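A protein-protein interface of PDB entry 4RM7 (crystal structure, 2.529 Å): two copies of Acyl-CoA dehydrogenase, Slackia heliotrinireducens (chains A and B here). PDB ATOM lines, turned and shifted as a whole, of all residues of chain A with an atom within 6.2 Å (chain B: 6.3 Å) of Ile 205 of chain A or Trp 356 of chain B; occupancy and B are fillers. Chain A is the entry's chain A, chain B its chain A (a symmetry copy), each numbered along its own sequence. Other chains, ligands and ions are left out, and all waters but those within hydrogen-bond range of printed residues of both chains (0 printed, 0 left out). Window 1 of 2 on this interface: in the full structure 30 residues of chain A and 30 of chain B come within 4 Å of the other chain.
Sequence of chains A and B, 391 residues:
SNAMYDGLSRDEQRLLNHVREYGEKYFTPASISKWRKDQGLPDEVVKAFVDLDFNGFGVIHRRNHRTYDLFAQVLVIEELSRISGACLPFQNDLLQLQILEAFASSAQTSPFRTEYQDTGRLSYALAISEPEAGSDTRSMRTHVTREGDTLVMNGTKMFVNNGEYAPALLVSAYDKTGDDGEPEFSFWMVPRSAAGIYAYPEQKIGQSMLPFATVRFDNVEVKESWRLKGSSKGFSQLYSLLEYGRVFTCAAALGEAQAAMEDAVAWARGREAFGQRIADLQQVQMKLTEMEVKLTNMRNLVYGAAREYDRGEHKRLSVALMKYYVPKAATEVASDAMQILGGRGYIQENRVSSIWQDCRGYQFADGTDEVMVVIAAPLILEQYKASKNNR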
ATOM      1  N   GLN A 203      13.785   5.287   5.663  1.00  0.00           N
ATOM      2  CA  GLN A 203      14.117   6.141   4.519  1.00  0.00           C
ATOM      3  C   GLN A 203      14.229   7.624   4.916  1.00  0.00           C
ATOM      4  O   GLN A 203      13.253   8.242   5.328  1.00  0.00           O
ATOM      5  CB  GLN A 203      13.087   5.963   3.398  1.00  0.00           C
ATOM      6  CG  GLN A 203      11.643   5.930   3.881  1.00  0.00           C
ATOM      7  CD  GLN A 203      10.646   6.176   2.759  1.00  0.00           C
ATOM      8  OE1 GLN A 203      11.010   6.178   1.580  1.00  0.00           O
ATOM      9  NE2 GLN A 203       9.383   6.394   3.122  1.00  0.00           N
ATOM     10  N   LYS A 204      15.405   8.211   4.775  1.00  0.00           N
ATOM     11  CA  LYS A 204      15.584   9.610   5.111  1.00  0.00           C
ATOM     12  C   LYS A 204      15.434  10.483   3.887  1.00  0.00           C
ATOM     13  O   LYS A 204      15.496   9.991   2.790  1.00  0.00           O
ATOM     14  CB  LYS A 204      16.947   9.837   5.723  1.00  0.00           C
ATOM     15  CG  LYS A 204      17.449   8.706   6.568  1.00  0.00           C
ATOM     16  CD  LYS A 204      18.656   8.082   5.910  1.00  0.00           C
ATOM     17  CE  LYS A 204      19.934   8.770   6.313  1.00  0.00           C
ATOM     18  NZ  LYS A 204      21.081   7.976   5.820  1.00  0.00           N
ATOM     19  N   ILE A 205      15.228  11.779   4.078  1.00  0.00           N
ATOM     20  CA  ILE A 205      14.989  12.685   2.952  1.00  0.00           C
ATOM     21  C   ILE A 205      16.299  13.008   2.222  1.00  0.00           C
ATOM     22  O   ILE A 205      16.286  13.522   1.104  1.00  0.00           O
ATOM     23  CB  ILE A 205      14.306  14.015   3.398  1.00  0.00           C
ATOM     24  CG1 ILE A 205      15.284  14.868   4.217  1.00  0.00           C
ATOM     25  CG2 ILE A 205      13.022  13.739   4.164  1.00  0.00           C
ATOM     26  CD1 ILE A 205      14.734  16.183   4.686  1.00  0.00           C
ATOM     27  N   GLY A 206      17.428  12.708   2.857  1.00  0.00           N
ATOM     28  CA  GLY A 206      18.723  12.929   2.243  1.00  0.00           C
ATOM     29  C   GLY A 206      19.711  11.845   2.617  1.00  0.00           C
ATOM     30  O   GLY A 206      19.381  10.952   3.401  1.00  0.00           O
ATOM     31  N   GLN A 207      20.916  11.926   2.055  1.00  0.00           N
ATOM     32  CA  GLN A 207      21.991  10.957   2.298  1.00  0.00           C
ATOM     33  C   GLN A 207      21.585   9.551   1.905  1.00  0.00           C
ATOM     34  O   GLN A 207      21.758   8.619   2.681  1.00  0.00           O
ATOM     35  CB  GLN A 207      22.423  10.983   3.766  1.00  0.00           C
ATOM     36  CG  GLN A 207      22.900  12.354   4.203  1.00  0.00           C
ATOM     37  CD  GLN A 207      23.185  12.425   5.673  1.00  0.00           C
ATOM     38  OE1 GLN A 207      23.120  11.411   6.380  1.00  0.00           O
ATOM     39  NE2 GLN A 207      23.505  13.621   6.155  1.00  0.00           N
ATOM     40  N   SER A 208      21.058   9.426   0.691  1.00  0.00           N
ATOM     41  CA  SER A 208      20.521   8.181   0.146  1.00  0.00           C
ATOM     42  C   SER A 208      21.502   7.005   0.169  1.00  0.00           C
ATOM     43  O   SER A 208      21.098   5.860   0.349  1.00  0.00           O
ATOM     44  CB  SER A 208      20.050   8.424  -1.286  1.00  0.00           C
ATOM     45  OG  SER A 208      18.956   9.335  -1.310  1.00  0.00           O
ATOM     46  N   THR A 331      24.362  24.082   5.621  1.00  0.00           N
ATOM     47  CA  THR A 331      22.983  24.076   5.149  1.00  0.00           C
ATOM     48  C   THR A 331      22.609  25.445   4.593  1.00  0.00           C
ATOM     49  O   THR A 331      21.921  25.538   3.588  1.00  0.00           O
ATOM     50  CB  THR A 331      21.993  23.669   6.265  1.00  0.00           C
ATOM     51  OG1 THR A 331      22.379  22.399   6.790  1.00  0.00           O
ATOM     52  CG2 THR A 331      20.586  23.539   5.718  1.00  0.00           C
ATOM     53  N   TRP A 356      21.598  20.346  -0.105  1.00  0.00           N
ATOM     54  CA  TRP A 356      20.880  21.056   0.937  1.00  0.00           C
ATOM     55  C   TRP A 356      20.256  20.073   1.914  1.00  0.00           C
ATOM     56  O   TRP A 356      20.333  20.236   3.122  1.00  0.00           O
ATOM     57  CB  TRP A 356      19.818  21.945   0.291  1.00  0.00           C
ATOM     58  CG  TRP A 356      18.915  22.632   1.210  1.00  0.00           C
ATOM     59  CD1 TRP A 356      19.245  23.621   2.108  1.00  0.00           C
ATOM     60  CD2 TRP A 356      17.490  22.464   1.298  1.00  0.00           C
ATOM     61  NE1 TRP A 356      18.108  24.054   2.761  1.00  0.00           N
ATOM     62  CE2 TRP A 356      17.020  23.369   2.281  1.00  0.00           C
ATOM     63  CE3 TRP A 356      16.570  21.632   0.652  1.00  0.00           C
ATOM     64  CZ2 TRP A 356      15.669  23.465   2.626  1.00  0.00           C
ATOM     65  CZ3 TRP A 356      15.227  21.715   1.007  1.00  0.00           C
ATOM     66  CH2 TRP A 356      14.792  22.622   1.989  1.00  0.00           C
ATOM     67  N   GLN A 357      19.633  19.044   1.371  1.00  0.00           N
ATOM     68  CA  GLN A 357      19.055  17.992   2.189  1.00  0.00           C
ATOM     69  C   GLN A 357      20.106  17.209   2.970  1.00  0.00           C
ATOM     70  O   GLN A 357      19.911  16.939   4.144  1.00  0.00           O
ATOM     71  CB  GLN A 357      18.241  17.054   1.310  1.00  0.00           C
ATOM     72  CG  GLN A 357      16.998  17.718   0.735  1.00  0.00           C
ATOM     73  CD  GLN A 357      16.275  16.839  -0.270  1.00  0.00           C
ATOM     74  OE1 GLN A 357      16.872  16.001  -0.952  1.00  0.00           O
ATOM     75  NE2 GLN A 357      14.988  17.032  -0.370  1.00  0.00           N
ATOM     76  N   ASP A 358      21.203  16.837   2.316  1.00  0.00           N
ATOM     77  CA  ASP A 358      22.325  16.184   2.993  1.00  0.00           C
ATOM     78  C   ASP A 358      22.790  17.020   4.173  1.00  0.00           C
ATOM     79  O   ASP A 358      22.916  16.531   5.311  1.00  0.00           O
ATOM     80  CB  ASP A 358      23.516  15.960   2.051  1.00  0.00           C
ATOM     81  CG  ASP A 358      23.234  14.940   0.964  1.00  0.00           C
ATOM     82  OD1 ASP A 358      22.309  14.111   1.116  1.00  0.00           O
ATOM     83  OD2 ASP A 358      23.956  14.963  -0.053  1.00  0.00           O
ATOM     84  N   ARG A 360      21.418  19.368   5.899  1.00  0.00           N
ATOM     85  CA  ARG A 360      20.444  19.445   6.982  1.00  0.00           C
ATOM     86  C   ARG A 360      20.564  18.235   7.883  1.00  0.00           C
ATOM     87  O   ARG A 360      20.389  18.348   9.085  1.00  0.00           O
ATOM     88  CB  ARG A 360      19.016  19.538   6.442  1.00  0.00           C
ATOM     89  CG  ARG A 360      17.957  19.703   7.528  1.00  0.00           C
ATOM     90  CD  ARG A 360      18.049  21.088   8.152  1.00  0.00           C
ATOM     91  NE  ARG A 360      17.229  21.272   9.363  1.00  0.00           N
ATOM     92  CZ  ARG A 360      17.465  20.685  10.536  1.00  0.00           C
ATOM     93  NH1 ARG A 360      18.479  19.833  10.668  1.00  0.00           N
ATOM     94  NH2 ARG A 360      16.668  20.926  11.572  1.00  0.00           N
ATOM     95  N   GLU B 256       0.896  25.183   6.652  1.00  0.00           N
ATOM     96  CA  GLU B 256       1.796  24.046   6.766  1.00  0.00           C
ATOM     97  C   GLU B 256       2.731  24.247   7.960  1.00  0.00           C
ATOM     98  O   GLU B 256       2.975  23.314   8.728  1.00  0.00           O
ATOM     99  CB  GLU B 256       2.596  23.847   5.485  1.00  0.00           C
ATOM    100  CG  GLU B 256       1.757  23.483   4.289  1.00  0.00           C
ATOM    101  CD  GLU B 256       2.591  22.859   3.181  1.00  0.00           C
ATOM    102  OE1 GLU B 256       2.713  23.467   2.093  1.00  0.00           O
ATOM    103  OE2 GLU B 256       3.119  21.750   3.392  1.00  0.00           O
ATOM    104  N   ALA B 330       8.282  30.563   7.412  1.00  0.00           N
ATOM    105  CA  ALA B 330       7.650  29.255   7.468  1.00  0.00           C
ATOM    106  C   ALA B 330       8.705  28.136   7.425  1.00  0.00           C
ATOM    107  O   ALA B 330       8.598  27.142   8.157  1.00  0.00           O
ATOM    108  CB  ALA B 330       6.662  29.097   6.348  1.00  0.00           C
ATOM    109  N   THR B 331       9.725  28.314   6.586  1.00  0.00           N
ATOM    110  CA  THR B 331      10.771  27.310   6.437  1.00  0.00           C
ATOM    111  C   THR B 331      11.547  27.159   7.741  1.00  0.00           C
ATOM    112  O   THR B 331      11.902  26.056   8.127  1.00  0.00           O
ATOM    113  CB  THR B 331      11.740  27.651   5.282  1.00  0.00           C
ATOM    114  OG1 THR B 331      10.990  27.815   4.078  1.00  0.00           O
ATOM    115  CG2 THR B 331      12.734  26.529   5.061  1.00  0.00           C
ATOM    116  N   GLU B 332      11.782  28.268   8.425  1.00  0.00           N
ATOM    117  CA  GLU B 332      12.534  28.256   9.680  1.00  0.00           C
ATOM    118  C   GLU B 332      11.749  27.545  10.792  1.00  0.00           C
ATOM    119  O   GLU B 332      12.323  26.758  11.572  1.00  0.00           O
ATOM    120  CB  GLU B 332      12.903  29.687  10.091  1.00  0.00           C
ATOM    121  CG  GLU B 332      13.799  30.376   9.070  1.00  0.00           C
ATOM    122  CD  GLU B 332      14.132  31.828   9.403  1.00  0.00           C
ATOM    123  OE1 GLU B 332      13.599  32.368  10.404  1.00  0.00           O
ATOM    124  OE2 GLU B 332      14.942  32.418   8.653  1.00  0.00           O
ATOM    125  N   ALA B 334       9.413  25.191  10.290  1.00  0.00           N
ATOM    126  CA  ALA B 334       9.417  23.776   9.968  1.00  0.00           C
ATOM    127  C   ALA B 334      10.776  23.135  10.315  1.00  0.00           C
ATOM    128  O   ALA B 334      10.833  22.042  10.877  1.00  0.00           O
ATOM    129  CB  ALA B 334       9.081  23.582   8.512  1.00  0.00           C
ATOM    130  N   SER B 335      11.864  23.837  10.009  1.00  0.00           N
ATOM    131  CA  SER B 335      13.201  23.353  10.335  1.00  0.00           C
ATOM    132  C   SER B 335      13.424  23.193  11.850  1.00  0.00           C
ATOM    133  O   SER B 335      14.001  22.185  12.296  1.00  0.00           O
ATOM    134  CB  SER B 335      14.258  24.289   9.754  1.00  0.00           C
ATOM    135  OG  SER B 335      15.556  23.747   9.959  1.00  0.00           O
ATOM    136  N   ASP B 336      12.977  24.187  12.624  1.00  0.00           N
ATOM    137  CA  ASP B 336      13.014  24.125  14.090  1.00  0.00           C
ATOM    138  C   ASP B 336      12.181  22.976  14.629  1.00  0.00           C
ATOM    139  O   ASP B 336      12.569  22.324  15.609  1.00  0.00           O
ATOM    140  CB  ASP B 336      12.525  25.432  14.724  1.00  0.00           C
ATOM    141  CG  ASP B 336      13.583  26.525  14.706  1.00  0.00           C
ATOM    142  OD1 ASP B 336      14.773  26.184  14.870  1.00  0.00           O
ATOM    143  OD2 ASP B 336      13.222  27.719  14.513  1.00  0.00           O
ATOM    144  N   MET B 338      11.671  20.153  12.957  1.00  0.00           N
ATOM    145  CA  MET B 338      12.501  18.969  12.727  1.00  0.00           C
ATOM    146  C   MET B 338      13.531  18.813  13.823  1.00  0.00           C
ATOM    147  O   MET B 338      13.744  17.711  14.311  1.00  0.00           O
ATOM    148  CB  MET B 338      13.231  19.025  11.395  1.00  0.00           C
ATOM    149  CG  MET B 338      12.388  18.728  10.188  1.00  0.00           C
ATOM    150  SD  MET B 338      13.395  19.140   8.573  1.00  0.00           S
ATOM    151  CE  MET B 338      14.862  17.906   8.957  1.00  0.00           C
ATOM    152  N   GLY B 345      12.239  12.018  11.815  1.00  0.00           N
ATOM    153  CA  GLY B 345      11.763  13.324  11.397  1.00  0.00           C
ATOM    154  C   GLY B 345      12.753  14.062  10.494  1.00  0.00           C
ATOM    155  O   GLY B 345      12.496  15.192  10.048  1.00  0.00           O
ATOM    156  N   TYR B 346      13.900  13.427  10.251  1.00  0.00           N
ATOM    157  CA  TYR B 346      14.664  13.655   9.026  1.00  0.00           C
ATOM    158  C   TYR B 346      14.348  12.448   8.127  1.00  0.00           C
ATOM    159  O   TYR B 346      14.959  12.224   7.073  1.00  0.00           O
ATOM    160  CB  TYR B 346      16.159  13.798   9.325  1.00  0.00           C
ATOM    161  CG  TYR B 346      17.067  13.920   8.115  1.00  0.00           C
ATOM    162  CD1 TYR B 346      17.111  15.091   7.347  1.00  0.00           C
ATOM    163  CD2 TYR B 346      17.909  12.861   7.757  1.00  0.00           C
ATOM    164  CE1 TYR B 346      17.969  15.194   6.244  1.00  0.00           C
ATOM    165  CE2 TYR B 346      18.762  12.942   6.657  1.00  0.00           C
ATOM    166  CZ  TYR B 346      18.796  14.100   5.904  1.00  0.00           C
ATOM    167  OH  TYR B 346      19.666  14.145   4.827  1.00  0.00           O
ATOM    168  N   ILE B 347      13.367  11.674   8.585  1.00  0.00           N
ATOM    169  CA  ILE B 347      12.878  10.494   7.889  1.00  0.00           C
ATOM    170  C   ILE B 347      11.726  10.919   6.975  1.00  0.00           C
ATOM    171  O   ILE B 347      10.914  11.765   7.342  1.00  0.00           O
ATOM    172  CB  ILE B 347      12.432   9.402   8.897  1.00  0.00           C
ATOM    173  CG1 ILE B 347      13.564   9.111   9.883  1.00  0.00           C
ATOM    174  CG2 ILE B 347      12.024   8.124   8.200  1.00  0.00           C
ATOM    175  CD1 ILE B 347      13.173   8.151  10.972  1.00  0.00           C
ATOM    176  N   GLN B 348      11.676  10.344   5.779  1.00  0.00           N
ATOM    177  CA  GLN B 348      10.712  10.744   4.757  1.00  0.00           C
ATOM    178  C   GLN B 348       9.273  10.542   5.223  1.00  0.00           C
ATOM    179  O   GLN B 348       8.364  11.265   4.803  1.00  0.00           O
ATOM    180  CB  GLN B 348      10.967   9.961   3.468  1.00  0.00           C
ATOM    181  CG  GLN B 348      10.764  10.772   2.208  1.00  0.00           C
ATOM    182  CD  GLN B 348      11.414  10.130   0.998  1.00  0.00           C
ATOM    183  OE1 GLN B 348      11.485   8.905   0.896  1.00  0.00           O
ATOM    184  NE2 GLN B 348      11.899  10.957   0.077  1.00  0.00           N
ATOM    185  N   GLU B 349       9.090   9.563   6.104  1.00  0.00           N
ATOM    186  CA  GLU B 349       7.787   9.228   6.665  1.00  0.00           C
ATOM    187  C   GLU B 349       7.181  10.416   7.416  1.00  0.00           C
ATOM    188  O   GLU B 349       5.996  10.720   7.262  1.00  0.00           O
ATOM    189  CB  GLU B 349       7.920   8.014   7.588  1.00  0.00           C
ATOM    190  CG  GLU B 349       8.758   6.880   6.979  1.00  0.00           C
ATOM    191  CD  GLU B 349       9.054   5.740   7.955  1.00  0.00           C
ATOM    192  OE1 GLU B 349       8.351   5.627   8.986  1.00  0.00           O
ATOM    193  OE2 GLU B 349       9.996   4.957   7.684  1.00  0.00           O
ATOM    194  N   ASN B 350       8.005  11.092   8.212  1.00  0.00           N
ATOM    195  CA  ASN B 350       7.555  12.241   8.998  1.00  0.00           C
ATOM    196  C   ASN B 350       7.108  13.446   8.171  1.00  0.00           C
ATOM    197  O   ASN B 350       7.824  13.909   7.280  1.00  0.00           O
ATOM    198  CB  ASN B 350       8.653  12.691   9.939  1.00  0.00           C
ATOM    199  CG  ASN B 350       8.104  13.183  11.230  1.00  0.00           C
ATOM    200  OD1 ASN B 350       7.531  14.277  11.292  1.00  0.00           O
ATOM    201  ND2 ASN B 350       8.233  12.364  12.282  1.00  0.00           N
ATOM    202  N   ARG B 351       5.924  13.963   8.466  1.00  0.00           N
ATOM    203  CA  ARG B 351       5.392  15.016   7.626  1.00  0.00           C
ATOM    204  C   ARG B 351       6.151  16.320   7.824  1.00  0.00           C
ATOM    205  O   ARG B 351       6.175  17.142   6.921  1.00  0.00           O
ATOM    206  CB  ARG B 351       3.895  15.217   7.867  1.00  0.00           C
ATOM    207  CG  ARG B 351       3.505  15.857   9.162  1.00  0.00           C
ATOM    208  CD  ARG B 351       1.982  15.969   9.225  1.00  0.00           C
ATOM    209  NE  ARG B 351       1.558  16.816  10.335  1.00  0.00           N
ATOM    210  CZ  ARG B 351       0.323  17.279  10.493  1.00  0.00           C
ATOM    211  NH1 ARG B 351      -0.624  17.010   9.596  1.00  0.00           N
ATOM    212  NH2 ARG B 351       0.039  18.025  11.545  1.00  0.00           N
ATOM    213  N   VAL B 352       6.811  16.493   8.966  1.00  0.00           N
ATOM    214  CA  VAL B 352       7.569  17.724   9.203  1.00  0.00           C
ATOM    215  C   VAL B 352       8.678  17.937   8.149  1.00  0.00           C
ATOM    216  O   VAL B 352       8.915  19.055   7.700  1.00  0.00           O
ATOM    217  CB  VAL B 352       8.167  17.759  10.635  1.00  0.00           C
ATOM    218  CG1 VAL B 352       9.085  18.910  10.773  1.00  0.00           C
ATOM    219  CG2 VAL B 352       7.071  17.973  11.646  1.00  0.00           C
ATOM    220  N   SER B 353       9.324  16.866   7.721  1.00  0.00           N
ATOM    221  CA  SER B 353      10.339  16.965   6.675  1.00  0.00           C
ATOM    222  C   SER B 353       9.751  17.285   5.284  1.00  0.00           C
ATOM    223  O   SER B 353      10.419  17.917   4.471  1.00  0.00           O
ATOM    224  CB  SER B 353      11.164  15.669   6.615  1.00  0.00           C
ATOM    225  OG  SER B 353      10.344  14.528   6.408  1.00  0.00           O
ATOM    226  N   SER B 354       8.522  16.853   5.002  1.00  0.00           N
ATOM    227  CA  SER B 354       7.842  17.274   3.776  1.00  0.00           C
ATOM    228  C   SER B 354       7.468  18.735   3.881  1.00  0.00           C
ATOM    229  O   SER B 354       7.631  19.499   2.931  1.00  0.00           O
ATOM    230  CB  SER B 354       6.577  16.473   3.513  1.00  0.00           C
ATOM    231  OG  SER B 354       6.764  15.122   3.848  1.00  0.00           O
ATOM    232  N   ILE B 355       6.944  19.123   5.039  1.00  0.00           N
ATOM    233  CA  ILE B 355       6.544  20.497   5.254  1.00  0.00           C
ATOM    234  C   ILE B 355       7.725  21.434   5.026  1.00  0.00           C
ATOM    235  O   ILE B 355       7.613  22.455   4.361  1.00  0.00           O
ATOM    236  CB  ILE B 355       5.994  20.675   6.657  1.00  0.00           C
ATOM    237  CG1 ILE B 355       4.638  19.972   6.763  1.00  0.00           C
ATOM    238  CG2 ILE B 355       5.927  22.184   7.039  1.00  0.00           C
ATOM    239  CD1 ILE B 355       4.108  19.902   8.203  1.00  0.00           C
ATOM    240  N   TRP B 356       8.868  21.059   5.570  1.00  0.00           N
ATOM    241  CA  TRP B 356      10.080  21.849   5.447  1.00  0.00           C
ATOM    242  C   TRP B 356      10.442  22.037   3.983  1.00  0.00           C
ATOM    243  O   TRP B 356      10.778  23.127   3.543  1.00  0.00           O
ATOM    244  CB  TRP B 356      11.205  21.152   6.210  1.00  0.00           C
ATOM    245  CG  TRP B 356      12.531  21.748   6.079  1.00  0.00           C
ATOM    246  CD1 TRP B 356      12.932  22.980   6.543  1.00  0.00           C
ATOM    247  CD2 TRP B 356      13.697  21.130   5.510  1.00  0.00           C
ATOM    248  NE1 TRP B 356      14.274  23.165   6.270  1.00  0.00           N
ATOM    249  CE2 TRP B 356      14.768  22.048   5.644  1.00  0.00           C
ATOM    250  CE3 TRP B 356      13.938  19.899   4.890  1.00  0.00           C
ATOM    251  CZ2 TRP B 356      16.057  21.767   5.186  1.00  0.00           C
ATOM    252  CZ3 TRP B 356      15.217  19.626   4.417  1.00  0.00           C
ATOM    253  CH2 TRP B 356      16.259  20.558   4.564  1.00  0.00           C
ATOM    254  N   GLN B 357      10.370  20.956   3.231  1.00  0.00           N
ATOM    255  CA  GLN B 357      10.619  21.010   1.802  1.00  0.00           C
ATOM    256  C   GLN B 357       9.587  21.850   1.055  1.00  0.00           C
ATOM    257  O   GLN B 357       9.953  22.639   0.200  1.00  0.00           O
ATOM    258  CB  GLN B 357      10.658  19.597   1.238  1.00  0.00           C
ATOM    259  CG  GLN B 357      11.857  18.801   1.731  1.00  0.00           C
ATOM    260  CD  GLN B 357      11.811  17.344   1.305  1.00  0.00           C
ATOM    261  OE1 GLN B 357      10.744  16.755   1.111  1.00  0.00           O
ATOM    262  NE2 GLN B 357      12.969  16.757   1.163  1.00  0.00           N
ATOM    263  N   ASP B 358       8.307  21.667   1.369  1.00  0.00           N
ATOM    264  CA  ASP B 358       7.244  22.498   0.800  1.00  0.00           C
ATOM    265  C   ASP B 358       7.539  23.970   1.036  1.00  0.00           C
ATOM    266  O   ASP B 358       7.524  24.796   0.105  1.00  0.00           O
ATOM    267  CB  ASP B 358       5.871  22.170   1.405  1.00  0.00           C
ATOM    268  CG  ASP B 358       5.363  20.794   1.022  1.00  0.00           C
ATOM    269  OD1 ASP B 358       5.827  20.221   0.010  1.00  0.00           O
ATOM    270  OD2 ASP B 358       4.480  20.282   1.738  1.00  0.00           O
ATOM    271  N   CYS B 359       7.797  24.317   2.291  1.00  0.00           N
ATOM    272  CA  CYS B 359       7.943  25.734   2.621  1.00  0.00           C
ATOM    273  C   CYS B 359       9.145  26.363   1.915  1.00  0.00           C
ATOM    274  O   CYS B 359       9.078  27.502   1.474  1.00  0.00           O
ATOM    275  CB  CYS B 359       8.032  25.908   4.119  1.00  0.00           C
ATOM    276  SG  CYS B 359       6.433  25.571   4.940  1.00  0.00           S
ATOM    277  N   ARG B 360      10.223  25.601   1.752  1.00  0.00           N
ATOM    278  CA  ARG B 360      11.383  26.090   1.015  1.00  0.00           C
ATOM    279  C   ARG B 360      10.989  26.468  -0.396  1.00  0.00           C
ATOM    280  O   ARG B 360      11.515  27.423  -0.943  1.00  0.00           O
ATOM    281  CB  ARG B 360      12.496  25.043   0.971  1.00  0.00           C
ATOM    282  CG  ARG B 360      13.769  25.528   0.283  1.00  0.00           C
ATOM    283  CD  ARG B 360      14.475  26.564   1.144  1.00  0.00           C
ATOM    284  NE  ARG B 360      15.587  27.264   0.475  1.00  0.00           N
ATOM    285  CZ  ARG B 360      15.444  28.135  -0.524  1.00  0.00           C
ATOM    286  NH1 ARG B 360      14.236  28.399  -1.016  1.00  0.00           N
ATOM    287  NH2 ARG B 360      16.514  28.720  -1.052  1.00  0.00           N
ATOM    288  N   GLY B 361      10.058  25.713  -0.972  1.00  0.00           N
ATOM    289  CA  GLY B 361       9.562  25.964  -2.318  1.00  0.00           C
ATOM    290  C   GLY B 361       8.745  27.248  -2.437  1.00  0.00           C
ATOM    291  O   GLY B 361       8.776  27.943  -3.446  1.00  0.00           O
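The backbone carbonyl oxygen of Gln 203 of chain A sits at hydrogen-bond distance from the backbone NH of Gln 348 of chain B (2.7 Å).
O of Tyr 346 of chain B is in hydrogen-bond range of N of Ile 205 of chain A (3.0 Å).
The side-chain hydroxyl of Tyr 346 of chain B sits close to the backbone NH of Gly 206 of chain A, at 3.3 Å.
The backbone carbonyl oxygen (O) of Gln 357 of chain A lies within hydrogen-bond range of the side-chain hydroxyl (OH) of Tyr 346 of chain B (2.9 Å).
NE2 of Gln 357 of chain A lies close to NE2 of Gln 357 of chain B.
O of Ser 335 of chain B lies within hydrogen-bond range of NH2 of Arg 360 of chain A, 3.0 Å away.
The side-chain amide oxygen (OE1) of Gln 357 of chain A sits close to the backbone carbonyl oxygen (O) of Ile 205 of chain A.
OG1 of Thr 331 of chain B lies within hydrogen-bond range of N of Arg 360 of chain B, 3.3 Å away.
The backbone carbonyl oxygen (O) of Ile 347 of chain B is in hydrogen-bond range of the side-chain hydroxyl (OG) of Ser 353 of chain B (3.0 Å).
Among the printed residues, pairs that only touch across the chains: Gln 203 of chain A with Ile 347 of chain B (3.1 Å), Gln 203 of chain A with Glu 349 of chain B (3.9 Å), Lys 204 of chain A with Tyr 346 of chain B (3.3 Å), Lys 204 of chain A with Ile 347 of chain B (3.98 Å), Ile 205 of chain A with Gln 348 of chain B (3.8 Å), Ile 205 of chain A with Ser 353 of chain B (3.6 Å), Ile 205 of chain A with Trp 356 of chain B (3.5 Å), Ile 205 of chain A with Gln 357 of chain B (3.8 Å), Gln 207 of chain A with Tyr 346 of chain B (3.7 Å), Trp 356 of chain A with Trp 356 of chain B (3.1 Å), Trp 356 of chain A with Arg 360 of chain B (3.5 Å), Asp 358 of chain A with Tyr 346 of chain B (3.8 Å), Arg 360 of chain A with Met 338 of chain B (3.9 Å) and Arg 360 of chain A with Trp 356 of chain B (3.5 Å).
Of chain B, only Tyr 346, Gln 348, Ser 353, Trp 356 and Gln 357 come within 4 Å of Ile 205 of chain A.
Of chain A, only Ile 205 (3.5 Å), Trp 356 (3.1 Å) and Arg 360 (3.5 Å) come within 4 Å of Trp 356 of chain B.
Printed residues of chain B within 4 Å of Gln 203 of chain A: Ile 347 (3.1 Å), Gln 348 (2.7 Å) and Glu 349 (3.9 Å).
Of the printed residues of chain A, Glu 349 of chain B touches Gln 203.
Of the printed residues of chain B, Asp 358 of chain A touches Tyr 346.
Val 352 of chain B touches none of the printed residues of chain A.
The nearest residue of chain B that does not touch Ile 205 of chain A is Ile 347 of chain B (4.2 Å).
The nearest printed residue of chain B that does not touch Lys 204 of chain A is Gln 348 of chain B (4.03 Å).
Of the 11 printed residues of chain A, 9 touch a printed residue of chain B.
Printed residues of chain A that touch a printed residue of chain B: Gln 203, Lys 204, Ile 205, Gly 206, Gln 207, Trp 356, Gln 357, Asp 358 and Arg 360.
Hydrophobic or aromatic side chains of chain A within 4 Å of the printed part of chain B: Ile 205 and Trp 356.
Of the 25 printed residues of chain B, 10 touch a printed residue of chain A.
Hydrophobic or aromatic side chains of chain B within 4 Å of the printed part of chain A: Met 338, Tyr 346, Ile 347 and Trp 356.
Trp 356 of chain A touches its own counterpart, Trp 356 of chain B.
Trp 356 of chain A touches Arg 360 of chain B, and with the chains exchanged Arg 360 of chain A touches Trp 356 of chain B.
Gln 357 of chain A touches its own counterpart, Gln 357 of chain B.
Positions printed for both chains: 331, 356, 357, 358 and 360.
Of the 20 pairs that touch across the chains among the printed residues, 4 have their exchanged pair printed and touching as well.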
